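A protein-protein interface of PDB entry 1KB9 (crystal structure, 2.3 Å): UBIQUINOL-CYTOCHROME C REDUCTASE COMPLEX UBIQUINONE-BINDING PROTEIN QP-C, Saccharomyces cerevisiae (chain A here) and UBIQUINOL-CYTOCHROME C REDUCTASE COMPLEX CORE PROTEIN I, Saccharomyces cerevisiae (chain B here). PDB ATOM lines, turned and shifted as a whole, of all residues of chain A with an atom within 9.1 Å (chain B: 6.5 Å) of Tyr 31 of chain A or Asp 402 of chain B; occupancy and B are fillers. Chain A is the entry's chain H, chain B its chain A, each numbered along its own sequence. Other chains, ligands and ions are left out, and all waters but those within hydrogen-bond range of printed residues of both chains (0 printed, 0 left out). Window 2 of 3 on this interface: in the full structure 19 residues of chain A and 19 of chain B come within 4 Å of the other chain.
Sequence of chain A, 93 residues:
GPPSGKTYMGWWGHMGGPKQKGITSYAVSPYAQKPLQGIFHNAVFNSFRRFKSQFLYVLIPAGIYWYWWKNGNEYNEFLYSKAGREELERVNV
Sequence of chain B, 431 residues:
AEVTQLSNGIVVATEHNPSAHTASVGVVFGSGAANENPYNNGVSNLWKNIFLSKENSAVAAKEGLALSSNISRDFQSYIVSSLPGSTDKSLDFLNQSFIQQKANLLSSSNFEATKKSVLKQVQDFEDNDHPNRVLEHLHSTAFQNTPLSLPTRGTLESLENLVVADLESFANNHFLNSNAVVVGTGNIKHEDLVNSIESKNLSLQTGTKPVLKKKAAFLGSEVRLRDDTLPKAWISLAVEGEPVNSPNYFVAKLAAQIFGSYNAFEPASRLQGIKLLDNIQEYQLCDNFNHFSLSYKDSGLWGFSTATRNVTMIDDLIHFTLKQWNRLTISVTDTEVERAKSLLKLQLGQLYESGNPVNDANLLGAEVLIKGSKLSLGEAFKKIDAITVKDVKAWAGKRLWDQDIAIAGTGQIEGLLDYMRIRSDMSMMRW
The guanidinium group (NH1) of Arg 423 of chain B is in salt-bridge range of the side-chain carboxylate (OD1) of Asp 402 of chain B (2.6 Å). N of Asp 402 of chain B sits at hydrogen-bond distance from O of Met 426 of chain B, at 2.9 Å. The backbone carbonyl oxygen (O) of Gln 403 of chain B is in hydrogen-bond range of the guanidinium group (NE) of Arg 423 of chain B (3.2 Å). The side-chain carboxylate (OD2) of Asp 404 of chain B lies within salt-bridge range of the guanidinium group (NH2) of Arg 423 of chain B. The backbone carbonyl oxygen (O) of Met 420 of chain B is in hydrogen-bond range of the side-chain hydroxyl (OG) of Ser 424 of chain B. The side-chain hydroxyl of Ser 29 of chain A sits close to the backbone NH of Tyr 31 of chain A, 3.1 Å away.
Tyr 419 of chain B touches Ser 29 of chain A (CE2 to CB, 3.4 Å). Pro 30 of chain A touches Met 420 of chain B. Tyr 31 of chain A touches Asp 402 of chain B. Tyr 31 of chain A touches Asp 404 of chain B (CB to OD2, 3.5 Å). Tyr 31 of chain A touches Arg 423 of chain B.
The side-chain carboxylate (OD2) of Asp 404 of chain B lies within hydrogen-bond range of the side-chain hydroxyl (OG) of Ser 29 of chain A (2.7 Å).
Of the 14 printed residues of chain B, 5 touch a printed residue of chain A. Hydrophobic or aromatic side chains of chain B within 4 Å of the printed part of chain A: Tyr 419 and Met 420. Of the 8 printed residues of chain A, 3 touch a printed residue of chain B. Among the printed residues, 6 pairs touch across the chains. Among the printed residues, no Asp or Glu carboxylate lies within 4 Å of a Lys or Arg side-chain nitrogen of the other chain.
Printed residues of chain B within 4 Å of Pro 30 of chain A: Met 420. Of chain B, only Asp 402, Asp 404 and Arg 423 come within 4 Å of Tyr 31 of chain A. Gly 397 of chain B touches none of the printed residues of chain A. Of chain A, only Tyr 31 (3.8 Å) comes within 4 Å of Asp 402 of chain B. Of the printed residues of chain A, Asp 404 of chain B touches Ser 29 and Tyr 31. Of the printed residues of chain A, Tyr 419 of chain B touches Ser 29 (3.4 Å). The nearest residue of chain B that does not touch Tyr 31 of chain A is Met 420 of chain B (4.2 Å). The nearest residue of chain A that does not touch Asp 402 of chain B is Ser 29 of chain A (8.8 Å).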
ATOM      1  N   VAL A  28      10.974 -11.822 -12.997  1.00  0.00           N
ATOM      2  CA  VAL A  28      10.544 -13.169 -13.316  1.00  0.00           C
ATOM      3  C   VAL A  28       9.025 -13.269 -13.224  1.00  0.00           C
ATOM      4  O   VAL A  28       8.416 -12.796 -12.261  1.00  0.00           O
ATOM      5  CB  VAL A  28      11.197 -14.193 -12.342  1.00  0.00           C
ATOM      6  CG1 VAL A  28      10.571 -15.566 -12.510  1.00  0.00           C
ATOM      7  CG2 VAL A  28      12.696 -14.278 -12.606  1.00  0.00           C
ATOM      8  N   SER A  29       8.425 -13.912 -14.220  1.00  0.00           N
ATOM      9  CA  SER A  29       6.985 -14.083 -14.277  1.00  0.00           C
ATOM     10  C   SER A  29       6.380 -14.600 -12.982  1.00  0.00           C
ATOM     11  O   SER A  29       6.942 -15.482 -12.328  1.00  0.00           O
ATOM     12  CB  SER A  29       6.607 -15.046 -15.403  1.00  0.00           C
ATOM     13  OG  SER A  29       5.223 -15.367 -15.362  1.00  0.00           O
ATOM     14  N   PRO A  30       5.251 -14.003 -12.563  1.00  0.00           N
ATOM     15  CA  PRO A  30       4.548 -14.404 -11.345  1.00  0.00           C
ATOM     16  C   PRO A  30       4.102 -15.854 -11.494  1.00  0.00           C
ATOM     17  O   PRO A  30       3.906 -16.557 -10.506  1.00  0.00           O
ATOM     18  CB  PRO A  30       3.343 -13.466 -11.332  1.00  0.00           C
ATOM     19  CG  PRO A  30       3.915 -12.210 -11.913  1.00  0.00           C
ATOM     20  CD  PRO A  30       4.706 -12.736 -13.090  1.00  0.00           C
ATOM     21  N   TYR A  31       3.935 -16.290 -12.740  1.00  0.00           N
ATOM     22  CA  TYR A  31       3.515 -17.658 -13.029  1.00  0.00           C
ATOM     23  C   TYR A  31       4.578 -18.676 -12.630  1.00  0.00           C
ATOM     24  O   TYR A  31       4.258 -19.752 -12.123  1.00  0.00           O
ATOM     25  CB  TYR A  31       3.194 -17.818 -14.514  1.00  0.00           C
ATOM     26  CG  TYR A  31       1.857 -17.262 -14.922  1.00  0.00           C
ATOM     27  CD1 TYR A  31       1.736 -15.951 -15.395  1.00  0.00           C
ATOM     28  CD2 TYR A  31       0.714 -18.058 -14.877  1.00  0.00           C
ATOM     29  CE1 TYR A  31       0.508 -15.453 -15.821  1.00  0.00           C
ATOM     30  CE2 TYR A  31      -0.523 -17.567 -15.297  1.00  0.00           C
ATOM     31  CZ  TYR A  31      -0.618 -16.269 -15.772  1.00  0.00           C
ATOM     32  OH  TYR A  31      -1.835 -15.801 -16.228  1.00  0.00           O
ATOM     33  N   ALA A  32       5.840 -18.305 -12.834  1.00  0.00           N
ATOM     34  CA  ALA A  32       6.979 -19.158 -12.519  1.00  0.00           C
ATOM     35  C   ALA A  32       7.387 -19.091 -11.051  1.00  0.00           C
ATOM     36  O   ALA A  32       8.299 -19.803 -10.624  1.00  0.00           O
ATOM     37  CB  ALA A  32       8.161 -18.776 -13.395  1.00  0.00           C
ATOM     38  N   GLN A  33       6.729 -18.229 -10.284  1.00  0.00           N
ATOM     39  CA  GLN A  33       7.065 -18.070  -8.877  1.00  0.00           C
ATOM     40  C   GLN A  33       6.292 -18.980  -7.946  1.00  0.00           C
ATOM     41  O   GLN A  33       5.196 -19.444  -8.258  1.00  0.00           O
ATOM     42  CB  GLN A  33       6.913 -16.610  -8.443  1.00  0.00           C
ATOM     43  CG  GLN A  33       7.836 -15.658  -9.185  1.00  0.00           C
ATOM     44  CD  GLN A  33       7.760 -14.234  -8.665  1.00  0.00           C
ATOM     45  OE1 GLN A  33       7.528 -14.006  -7.474  1.00  0.00           O
ATOM     46  NE2 GLN A  33       7.971 -13.266  -9.551  1.00  0.00           N
ATOM     47  N   LYS A  34       6.903 -19.235  -6.796  1.00  0.00           N
ATOM     48  CA  LYS A  34       6.344 -20.091  -5.765  1.00  0.00           C
ATOM     49  C   LYS A  34       5.015 -19.508  -5.292  1.00  0.00           C
ATOM     50  O   LYS A  34       4.969 -18.384  -4.785  1.00  0.00           O
ATOM     51  CB  LYS A  34       7.350 -20.180  -4.612  1.00  0.00           C
ATOM     52  CG  LYS A  34       7.212 -21.385  -3.697  1.00  0.00           C
ATOM     53  CD  LYS A  34       8.588 -21.838  -3.209  1.00  0.00           C
ATOM     54  CE  LYS A  34       9.403 -20.676  -2.635  1.00  0.00           C
ATOM     55  NZ  LYS A  34      10.807 -21.062  -2.307  1.00  0.00           N
ATOM     56  N   PRO A  35       3.911 -20.256  -5.483  1.00  0.00           N
ATOM     57  CA  PRO A  35       2.570 -19.818  -5.080  1.00  0.00           C
ATOM     58  C   PRO A  35       2.539 -19.309  -3.644  1.00  0.00           C
ATOM     59  O   PRO A  35       3.183 -19.869  -2.757  1.00  0.00           O
ATOM     60  CB  PRO A  35       1.718 -21.078  -5.274  1.00  0.00           C
ATOM     61  CG  PRO A  35       2.716 -22.205  -5.211  1.00  0.00           C
ATOM     62  CD  PRO A  35       3.874 -21.640  -5.979  1.00  0.00           C
ATOM     63  N   ASN B 326      -2.230 -14.342 -31.415  1.00  0.00           N
ATOM     64  CA  ASN B 326      -3.384 -14.987 -30.780  1.00  0.00           C
ATOM     65  C   ASN B 326      -4.168 -15.726 -31.851  1.00  0.00           C
ATOM     66  O   ASN B 326      -4.758 -16.777 -31.598  1.00  0.00           O
ATOM     67  CB  ASN B 326      -4.344 -13.968 -30.150  1.00  0.00           C
ATOM     68  CG  ASN B 326      -3.799 -13.308 -28.893  1.00  0.00           C
ATOM     69  OD1 ASN B 326      -4.247 -12.231 -28.529  1.00  0.00           O
ATOM     70  ND2 ASN B 326      -2.846 -13.949 -28.225  1.00  0.00           N
ATOM     71  N   ALA B 396       0.119 -23.761 -31.728  1.00  0.00           N
ATOM     72  CA  ALA B 396      -0.050 -22.453 -31.101  1.00  0.00           C
ATOM     73  C   ALA B 396      -0.780 -22.551 -29.765  1.00  0.00           C
ATOM     74  O   ALA B 396      -0.396 -21.900 -28.791  1.00  0.00           O
ATOM     75  CB  ALA B 396      -0.782 -21.524 -32.036  1.00  0.00           C
ATOM     76  N   GLY B 397      -1.798 -23.408 -29.711  1.00  0.00           N
ATOM     77  CA  GLY B 397      -2.562 -23.583 -28.489  1.00  0.00           C
ATOM     78  C   GLY B 397      -1.763 -24.203 -27.359  1.00  0.00           C
ATOM     79  O   GLY B 397      -2.192 -24.200 -26.201  1.00  0.00           O
ATOM     80  N   LEU B 400       1.963 -20.908 -27.670  1.00  0.00           N
ATOM     81  CA  LEU B 400       1.704 -19.471 -27.594  1.00  0.00           C
ATOM     82  C   LEU B 400       0.574 -19.020 -26.659  1.00  0.00           C
ATOM     83  O   LEU B 400       0.736 -18.052 -25.916  1.00  0.00           O
ATOM     84  CB  LEU B 400       1.433 -18.925 -28.995  1.00  0.00           C
ATOM     85  CG  LEU B 400       2.578 -18.461 -29.905  1.00  0.00           C
ATOM     86  CD1 LEU B 400       3.745 -19.421 -29.870  1.00  0.00           C
ATOM     87  CD2 LEU B 400       2.060 -18.341 -31.319  1.00  0.00           C
ATOM     88  N   TRP B 401      -0.546 -19.737 -26.673  1.00  0.00           N
ATOM     89  CA  TRP B 401      -1.708 -19.372 -25.874  1.00  0.00           C
ATOM     90  C   TRP B 401      -1.573 -19.426 -24.356  1.00  0.00           C
ATOM     91  O   TRP B 401      -1.522 -20.508 -23.760  1.00  0.00           O
ATOM     92  CB  TRP B 401      -2.936 -20.176 -26.312  1.00  0.00           C
ATOM     93  CG  TRP B 401      -4.248 -19.627 -25.790  1.00  0.00           C
ATOM     94  CD1 TRP B 401      -4.875 -19.966 -24.625  1.00  0.00           C
ATOM     95  CD2 TRP B 401      -5.090 -18.658 -26.430  1.00  0.00           C
ATOM     96  NE1 TRP B 401      -6.053 -19.270 -24.499  1.00  0.00           N
ATOM     97  CE2 TRP B 401      -6.211 -18.461 -25.594  1.00  0.00           C
ATOM     98  CE3 TRP B 401      -5.006 -17.937 -27.630  1.00  0.00           C
ATOM     99  CZ2 TRP B 401      -7.241 -17.576 -25.916  1.00  0.00           C
ATOM    100  CZ3 TRP B 401      -6.034 -17.051 -27.953  1.00  0.00           C
ATOM    101  CH2 TRP B 401      -7.137 -16.881 -27.096  1.00  0.00           C
ATOM    102  N   ASP B 402      -1.630 -18.243 -23.738  1.00  0.00           N
ATOM    103  CA  ASP B 402      -1.530 -18.092 -22.287  1.00  0.00           C
ATOM    104  C   ASP B 402      -0.283 -18.788 -21.741  1.00  0.00           C
ATOM    105  O   ASP B 402      -0.339 -19.544 -20.775  1.00  0.00           O
ATOM    106  CB  ASP B 402      -2.802 -18.623 -21.616  1.00  0.00           C
ATOM    107  CG  ASP B 402      -2.904 -18.241 -20.152  1.00  0.00           C
ATOM    108  OD1 ASP B 402      -2.305 -17.234 -19.730  1.00  0.00           O
ATOM    109  OD2 ASP B 402      -3.605 -18.956 -19.415  1.00  0.00           O
ATOM    110  N   GLN B 403       0.846 -18.498 -22.373  1.00  0.00           N
ATOM    111  CA  GLN B 403       2.131 -19.063 -21.997  1.00  0.00           C
ATOM    112  C   GLN B 403       3.083 -17.947 -21.600  1.00  0.00           C
ATOM    113  O   GLN B 403       2.980 -16.824 -22.104  1.00  0.00           O
ATOM    114  CB  GLN B 403       2.745 -19.828 -23.178  1.00  0.00           C
ATOM    115  CG  GLN B 403       2.015 -21.102 -23.548  1.00  0.00           C
ATOM    116  CD  GLN B 403       2.016 -22.121 -22.429  1.00  0.00           C
ATOM    117  OE1 GLN B 403       3.014 -22.294 -21.729  1.00  0.00           O
ATOM    118  NE2 GLN B 403       0.890 -22.808 -22.255  1.00  0.00           N
ATOM    119  N   ASP B 404       4.016 -18.268 -20.709  1.00  0.00           N
ATOM    120  CA  ASP B 404       5.010 -17.312 -20.255  1.00  0.00           C
ATOM    121  C   ASP B 404       5.846 -16.852 -21.424  1.00  0.00           C
ATOM    122  O   ASP B 404       5.973 -17.552 -22.416  1.00  0.00           O
ATOM    123  CB  ASP B 404       5.931 -17.951 -19.216  1.00  0.00           C
ATOM    124  CG  ASP B 404       5.459 -17.735 -17.799  1.00  0.00           C
ATOM    125  OD1 ASP B 404       5.915 -18.481 -16.900  1.00  0.00           O
ATOM    126  OD2 ASP B 404       4.664 -16.802 -17.576  1.00  0.00           O
ATOM    127  N   TYR B 419       5.900  -6.413 -17.414  1.00  0.00           N
ATOM    128  CA  TYR B 419       5.785  -7.800 -17.811  1.00  0.00           C
ATOM    129  C   TYR B 419       4.351  -8.293 -17.903  1.00  0.00           C
ATOM    130  O   TYR B 419       3.940  -8.774 -18.958  1.00  0.00           O
ATOM    131  CB  TYR B 419       6.585  -8.693 -16.859  1.00  0.00           C
ATOM    132  CG  TYR B 419       6.659 -10.134 -17.316  1.00  0.00           C
ATOM    133  CD1 TYR B 419       7.646 -10.550 -18.216  1.00  0.00           C
ATOM    134  CD2 TYR B 419       5.731 -11.081 -16.862  1.00  0.00           C
ATOM    135  CE1 TYR B 419       7.712 -11.871 -18.653  1.00  0.00           C
ATOM    136  CE2 TYR B 419       5.781 -12.401 -17.295  1.00  0.00           C
ATOM    137  CZ  TYR B 419       6.778 -12.791 -18.193  1.00  0.00           C
ATOM    138  OH  TYR B 419       6.831 -14.094 -18.634  1.00  0.00           O
ATOM    139  N   MET B 420       3.600  -8.181 -16.810  1.00  0.00           N
ATOM    140  CA  MET B 420       2.212  -8.645 -16.774  1.00  0.00           C
ATOM    141  C   MET B 420       1.281  -8.127 -17.863  1.00  0.00           C
ATOM    142  O   MET B 420       0.369  -8.842 -18.290  1.00  0.00           O
ATOM    143  CB  MET B 420       1.600  -8.435 -15.396  1.00  0.00           C
ATOM    144  CG  MET B 420       2.113  -9.450 -14.404  1.00  0.00           C
ATOM    145  SD  MET B 420       1.861 -11.150 -15.004  1.00  0.00           S
ATOM    146  CE  MET B 420       0.463 -11.642 -13.993  1.00  0.00           C
ATOM    147  N   ARG B 423       2.374 -10.108 -20.897  1.00  0.00           N
ATOM    148  CA  ARG B 423       1.966 -11.485 -20.652  1.00  0.00           C
ATOM    149  C   ARG B 423       0.452 -11.697 -20.802  1.00  0.00           C
ATOM    150  O   ARG B 423       0.018 -12.720 -21.332  1.00  0.00           O
ATOM    151  CB  ARG B 423       2.485 -11.938 -19.273  1.00  0.00           C
ATOM    152  CG  ARG B 423       1.999 -13.292 -18.772  1.00  0.00           C
ATOM    153  CD  ARG B 423       2.430 -14.466 -19.645  1.00  0.00           C
ATOM    154  NE  ARG B 423       1.337 -15.438 -19.730  1.00  0.00           N
ATOM    155  CZ  ARG B 423       1.277 -16.557 -19.019  1.00  0.00           C
ATOM    156  NH1 ARG B 423       0.247 -17.372 -19.126  1.00  0.00           N
ATOM    157  NH2 ARG B 423       2.279 -16.898 -18.238  1.00  0.00           N
ATOM    158  N   SER B 424      -0.342 -10.716 -20.379  1.00  0.00           N
ATOM    159  CA  SER B 424      -1.800 -10.802 -20.491  1.00  0.00           C
ATOM    160  C   SER B 424      -2.259 -10.865 -21.952  1.00  0.00           C
ATOM    161  O   SER B 424      -3.287 -11.464 -22.265  1.00  0.00           O
ATOM    162  CB  SER B 424      -2.458  -9.611 -19.788  1.00  0.00           C
ATOM    163  OG  SER B 424      -2.240  -9.679 -18.387  1.00  0.00           O
ATOM    164  N   MET B 426      -1.084 -12.585 -24.246  1.00  0.00           N
ATOM    165  CA  MET B 426      -0.828 -13.891 -24.845  1.00  0.00           C
ATOM    166  C   MET B 426      -2.126 -14.680 -25.000  1.00  0.00           C
ATOM    167  O   MET B 426      -2.100 -15.881 -25.279  1.00  0.00           O
ATOM    168  CB  MET B 426       0.180 -14.693 -24.016  1.00  0.00           C
ATOM    169  CG  MET B 426       1.568 -14.119 -24.020  1.00  0.00           C
ATOM    170  SD  MET B 426       2.178 -13.836 -25.686  1.00  0.00           S
ATOM    171  CE  MET B 426       2.760 -15.450 -26.095  1.00  0.00           C
ATOM    172  N   SER B 427      -3.253 -14.008 -24.780  1.00  0.00           N
ATOM    173  CA  SER B 427      -4.571 -14.626 -24.910  1.00  0.00           C
ATOM    174  C   SER B 427      -5.666 -13.582 -25.092  1.00  0.00           C
ATOM    175  O   SER B 427      -5.390 -12.384 -25.194  1.00  0.00           O
ATOM    176  CB  SER B 427      -4.887 -15.518 -23.708  1.00  0.00           C
ATOM    177  OG  SER B 427      -4.971 -14.773 -22.510  1.00  0.00           O
